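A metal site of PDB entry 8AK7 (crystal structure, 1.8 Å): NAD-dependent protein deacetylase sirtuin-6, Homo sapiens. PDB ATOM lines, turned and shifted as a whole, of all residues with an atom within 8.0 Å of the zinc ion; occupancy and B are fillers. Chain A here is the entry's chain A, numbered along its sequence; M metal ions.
The side-chain sulfur of Cys 138 lies close to the side-chain hydroxyl of Thr 140, 3.0 Å away.
N of Cys 135 is in hydrogen-bond range of O of Thr 140 (3.0 Å).
The backbone carbonyl oxygen (O) of Gly 173 is in hydrogen-bond range of the backbone NH (N) of Cys 160.
The backbone NH of Val 162 sits close to the side-chain sulfur of Cys 160.
SG of Cys 160 sits close to OH of Tyr 142 (2.9 Å).
O of Cys 160 is in hydrogen-bond range of N of Arg 172 (3.2 Å).
SG of Cys 171 lies close to N of Gly 173, at 3.4 Å.
The backbone NH (N) of Cys 171 is in hydrogen-bond range of the backbone carbonyl oxygen (O) of Val 162, at 3.2 Å.
Of the 19 residues printed, 4 come within 4 Å of the zinc ion.
The nearest printed residue that does not touch the zinc ion is Gly 173 (4.6 Å).
The side-chain sulfur (SG) of Cys 138 binds the zinc ion.
SG of Cys 135 binds the zinc ion.
The zinc ion is bound by SG of Cys 160 (2.3 Å).
SG of Cys 171 is bound to the zinc ion (2.4 Å).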
ATOM      1  N   GLU A 134     -29.932 -30.438  22.344  1.00  0.00           N
ATOM      2  CA  GLU A 134     -28.620 -29.782  22.595  1.00  0.00           C
ATOM      3  C   GLU A 134     -28.136 -29.153  21.293  1.00  0.00           C
ATOM      4  O   GLU A 134     -28.202 -29.821  20.247  1.00  0.00           O
ATOM      5  CB  GLU A 134     -27.658 -30.852  23.137  1.00  0.00           C
ATOM      6  CG  GLU A 134     -26.223 -30.401  23.263  1.00  0.00           C
ATOM      7  CD  GLU A 134     -25.337 -31.451  23.921  1.00  0.00           C
ATOM      8  OE1 GLU A 134     -25.802 -32.083  24.884  1.00  0.00           O
ATOM      9  OE2 GLU A 134     -24.210 -31.652  23.444  1.00  0.00           O
ATOM     10  N   CYS A 135     -27.656 -27.914  21.366  1.00  0.00           N
ATOM     11  CA  CYS A 135     -27.037 -27.192  20.221  1.00  0.00           C
ATOM     12  C   CYS A 135     -25.686 -27.845  19.926  1.00  0.00           C
ATOM     13  O   CYS A 135     -24.867 -27.939  20.861  1.00  0.00           O
ATOM     14  CB  CYS A 135     -26.824 -25.722  20.568  1.00  0.00           C
ATOM     15  SG  CYS A 135     -26.042 -24.737  19.260  1.00  0.00           S
ATOM     16  N   ALA A 136     -25.447 -28.260  18.691  1.00  0.00           N
ATOM     17  CA  ALA A 136     -24.141 -28.815  18.272  1.00  0.00           C
ATOM     18  C   ALA A 136     -23.026 -27.778  18.459  1.00  0.00           C
ATOM     19  O   ALA A 136     -21.929 -28.163  18.883  1.00  0.00           O
ATOM     20  CB  ALA A 136     -24.225 -29.288  16.853  1.00  0.00           C
ATOM     21  N   LYS A 137     -23.308 -26.506  18.166  1.00  0.00           N
ATOM     22  CA  LYS A 137     -22.261 -25.436  18.192  1.00  0.00           C
ATOM     23  C   LYS A 137     -21.910 -25.073  19.632  1.00  0.00           C
ATOM     24  O   LYS A 137     -20.727 -25.202  19.979  1.00  0.00           O
ATOM     25  CB  LYS A 137     -22.726 -24.175  17.466  1.00  0.00           C
ATOM     26  CG  LYS A 137     -22.879 -24.302  15.958  1.00  0.00           C
ATOM     27  CD  LYS A 137     -23.138 -22.962  15.315  1.00  0.00           C
ATOM     28  CE  LYS A 137     -23.274 -23.023  13.804  1.00  0.00           C
ATOM     29  NZ  LYS A 137     -23.647 -21.709  13.243  1.00  0.00           N
ATOM     30  N   CYS A 138     -22.882 -24.627  20.436  1.00  0.00           N
ATOM     31  CA  CYS A 138     -22.571 -24.033  21.761  1.00  0.00           C
ATOM     32  C   CYS A 138     -22.921 -24.986  22.916  1.00  0.00           C
ATOM     33  O   CYS A 138     -22.673 -24.591  24.070  1.00  0.00           O
ATOM     34  CB  CYS A 138     -23.259 -22.679  21.942  1.00  0.00           C
ATOM     35  SG  CYS A 138     -25.043 -22.756  22.206  1.00  0.00           S
ATOM     36  N   LYS A 139     -23.484 -26.162  22.636  1.00  0.00           N
ATOM     37  CA  LYS A 139     -23.769 -27.219  23.636  1.00  0.00           C
ATOM     38  C   LYS A 139     -24.934 -26.797  24.547  1.00  0.00           C
ATOM     39  O   LYS A 139     -25.295 -27.608  25.419  1.00  0.00           O
ATOM     40  CB  LYS A 139     -22.516 -27.556  24.448  1.00  0.00           C
ATOM     41  CG  LYS A 139     -21.295 -27.929  23.617  1.00  0.00           C
ATOM     42  CD  LYS A 139     -21.512 -29.102  22.692  1.00  0.00           C
ATOM     43  CE  LYS A 139     -20.280 -29.453  21.890  1.00  0.00           C
ATOM     44  NZ  LYS A 139     -20.557 -30.513  20.884  1.00  0.00           N
ATOM     45  N   THR A 140     -25.490 -25.596  24.377  1.00  0.00           N
ATOM     46  CA  THR A 140     -26.621 -25.144  25.221  1.00  0.00           C
ATOM     47  C   THR A 140     -27.720 -26.201  25.102  1.00  0.00           C
ATOM     48  O   THR A 140     -28.101 -26.532  23.973  1.00  0.00           O
ATOM     49  CB  THR A 140     -27.161 -23.759  24.844  1.00  0.00           C
ATOM     50  OG1 THR A 140     -26.105 -22.816  25.052  1.00  0.00           O
ATOM     51  CG2 THR A 140     -28.379 -23.375  25.653  1.00  0.00           C
ATOM     52  N   GLN A 141     -28.198 -26.710  26.240  1.00  0.00           N
ATOM     53  CA  GLN A 141     -29.286 -27.710  26.292  1.00  0.00           C
ATOM     54  C   GLN A 141     -30.621 -26.990  26.523  1.00  0.00           C
ATOM     55  O   GLN A 141     -30.645 -25.905  27.118  1.00  0.00           O
ATOM     56  CB  GLN A 141     -29.000 -28.765  27.348  1.00  0.00           C
ATOM     57  CG  GLN A 141     -27.872 -29.694  26.942  1.00  0.00           C
ATOM     58  CD  GLN A 141     -27.609 -30.772  27.961  1.00  0.00           C
ATOM     59  OE1 GLN A 141     -27.921 -30.605  29.139  1.00  0.00           O
ATOM     60  NE2 GLN A 141     -27.043 -31.875  27.519  1.00  0.00           N
ATOM     61  N   TYR A 142     -31.689 -27.576  25.992  1.00  0.00           N
ATOM     62  CA  TYR A 142     -33.068 -27.056  26.150  1.00  0.00           C
ATOM     63  C   TYR A 142     -33.937 -28.202  26.649  1.00  0.00           C
ATOM     64  O   TYR A 142     -33.981 -29.247  25.965  1.00  0.00           O
ATOM     65  CB  TYR A 142     -33.614 -26.535  24.828  1.00  0.00           C
ATOM     66  CG  TYR A 142     -32.838 -25.403  24.203  1.00  0.00           C
ATOM     67  CD1 TYR A 142     -31.684 -25.651  23.487  1.00  0.00           C
ATOM     68  CD2 TYR A 142     -33.283 -24.098  24.297  1.00  0.00           C
ATOM     69  CE1 TYR A 142     -30.974 -24.625  22.886  1.00  0.00           C
ATOM     70  CE2 TYR A 142     -32.585 -23.055  23.708  1.00  0.00           C
ATOM     71  CZ  TYR A 142     -31.413 -23.320  23.009  1.00  0.00           C
ATOM     72  OH  TYR A 142     -30.708 -22.326  22.408  1.00  0.00           O
ATOM     73  N   LEU A 159     -33.635 -24.592  15.857  1.00  0.00           N
ATOM     74  CA  LEU A 159     -32.314 -23.894  15.872  1.00  0.00           C
ATOM     75  C   LEU A 159     -32.084 -23.235  17.223  1.00  0.00           C
ATOM     76  O   LEU A 159     -33.072 -22.839  17.887  1.00  0.00           O
ATOM     77  CB  LEU A 159     -32.269 -22.841  14.755  1.00  0.00           C
ATOM     78  CG  LEU A 159     -32.377 -23.401  13.330  1.00  0.00           C
ATOM     79  CD1 LEU A 159     -32.362 -22.256  12.320  1.00  0.00           C
ATOM     80  CD2 LEU A 159     -31.246 -24.385  13.046  1.00  0.00           C
ATOM     81  N   CYS A 160     -30.812 -23.103  17.615  1.00  0.00           N
ATOM     82  CA  CYS A 160     -30.397 -22.496  18.900  1.00  0.00           C
ATOM     83  C   CYS A 160     -30.835 -21.024  18.942  1.00  0.00           C
ATOM     84  O   CYS A 160     -30.770 -20.357  17.881  1.00  0.00           O
ATOM     85  CB  CYS A 160     -28.889 -22.603  19.064  1.00  0.00           C
ATOM     86  SG  CYS A 160     -28.363 -22.213  20.745  1.00  0.00           S
ATOM     87  N   THR A 161     -31.303 -20.572  20.108  1.00  0.00           N
ATOM     88  CA  THR A 161     -31.899 -19.221  20.332  1.00  0.00           C
ATOM     89  C   THR A 161     -31.015 -18.392  21.265  1.00  0.00           C
ATOM     90  O   THR A 161     -31.494 -17.343  21.721  1.00  0.00           O
ATOM     91  CB  THR A 161     -33.329 -19.350  20.876  1.00  0.00           C
ATOM     92  OG1 THR A 161     -33.280 -19.961  22.160  1.00  0.00           O
ATOM     93  CG2 THR A 161     -34.244 -20.155  19.970  1.00  0.00           C
ATOM     94  N   VAL A 162     -29.787 -18.837  21.553  1.00  0.00           N
ATOM     95  CA  VAL A 162     -28.838 -18.106  22.442  1.00  0.00           C
ATOM     96  C   VAL A 162     -28.382 -16.831  21.715  1.00  0.00           C
ATOM     97  O   VAL A 162     -27.973 -16.958  20.539  1.00  0.00           O
ATOM     98  CB  VAL A 162     -27.646 -18.973  22.890  1.00  0.00           C
ATOM     99  CG1 VAL A 162     -26.616 -18.180  23.672  1.00  0.00           C
ATOM    100  CG2 VAL A 162     -28.111 -20.172  23.710  1.00  0.00           C
ATOM    101  N   ALA A 163     -28.453 -15.687  22.400  1.00  0.00           N
ATOM    102  CA  ALA A 163     -28.216 -14.322  21.877  1.00  0.00           C
ATOM    103  C   ALA A 163     -26.786 -14.203  21.323  1.00  0.00           C
ATOM    104  O   ALA A 163     -25.845 -14.237  22.143  1.00  0.00           O
ATOM    105  CB  ALA A 163     -28.455 -13.299  22.970  1.00  0.00           C
ATOM    106  N   CYS A 171     -26.706 -17.602  17.716  1.00  0.00           N
ATOM    107  CA  CYS A 171     -26.006 -18.890  17.452  1.00  0.00           C
ATOM    108  C   CYS A 171     -26.672 -19.593  16.275  1.00  0.00           C
ATOM    109  O   CYS A 171     -25.956 -19.951  15.316  1.00  0.00           O
ATOM    110  CB  CYS A 171     -26.053 -19.794  18.672  1.00  0.00           C
ATOM    111  SG  CYS A 171     -25.350 -21.436  18.357  1.00  0.00           S
ATOM    112  N   ARG A 172     -27.985 -19.824  16.380  1.00  0.00           N
ATOM    113  CA  ARG A 172     -28.812 -20.484  15.335  1.00  0.00           C
ATOM    114  C   ARG A 172     -28.209 -21.848  14.967  1.00  0.00           C
ATOM    115  O   ARG A 172     -28.474 -22.329  13.847  1.00  0.00           O
ATOM    116  CB  ARG A 172     -28.965 -19.559  14.122  1.00  0.00           C
ATOM    117  CG  ARG A 172     -29.288 -18.107  14.478  1.00  0.00           C
ATOM    118  CD  ARG A 172     -30.134 -17.372  13.457  1.00  0.00           C
ATOM    119  NE  ARG A 172     -29.999 -17.895  12.099  1.00  0.00           N
ATOM    120  CZ  ARG A 172     -30.942 -18.562  11.421  1.00  0.00           C
ATOM    121  NH1 ARG A 172     -32.130 -18.795  11.971  1.00  0.00           N
ATOM    122  NH2 ARG A 172     -30.693 -19.006  10.204  1.00  0.00           N
ATOM    123  N   GLY A 173     -27.476 -22.469  15.898  1.00  0.00           N
ATOM    124  CA  GLY A 173     -26.888 -23.803  15.706  1.00  0.00           C
ATOM    125  C   GLY A 173     -27.955 -24.873  15.571  1.00  0.00           C
ATOM    126  O   GLY A 173     -29.096 -24.632  16.020  1.00  0.00           O
ATOM    127  N   GLU A 174     -27.606 -26.003  14.945  1.00  0.00           N
ATOM    128  CA  GLU A 174     -28.512 -27.161  14.740  1.00  0.00           C
ATOM    129  C   GLU A 174     -28.758 -27.835  16.099  1.00  0.00           C
ATOM    130  O   GLU A 174     -27.765 -28.280  16.736  1.00  0.00           O
ATOM    131  CB  GLU A 174     -27.907 -28.100  13.700  1.00  0.00           C
ATOM    132  CG  GLU A 174     -28.712 -29.357  13.424  1.00  0.00           C
ATOM    133  CD  GLU A 174     -28.108 -30.287  12.384  1.00  0.00           C
ATOM    134  OE1 GLU A 174     -28.242 -29.982  11.188  1.00  0.00           O
ATOM    135  OE2 GLU A 174     -27.496 -31.311  12.778  1.00  0.00           O
ATOM    136  N   LEU A 175     -30.026 -27.876  16.551  1.00  0.00           N
ATOM    137  CA  LEU A 175     -30.432 -28.578  17.798  1.00  0.00           C
ATOM    138  C   LEU A 175     -30.620 -30.076  17.497  1.00  0.00           C
ATOM    139  O   LEU A 175     -31.316 -30.405  16.519  1.00  0.00           O
ATOM    140  CB  LEU A 175     -31.725 -27.964  18.357  1.00  0.00           C
ATOM    141  CG  LEU A 175     -31.617 -26.521  18.835  1.00  0.00           C
ATOM    142  CD1 LEU A 175     -32.905 -26.074  19.505  1.00  0.00           C
ATOM    143  CD2 LEU A 175     -30.434 -26.325  19.762  1.00  0.00           C
HETATM  144 ZN    ZN M   1     -26.135 -22.711  20.265  1.00  0.00          ZN
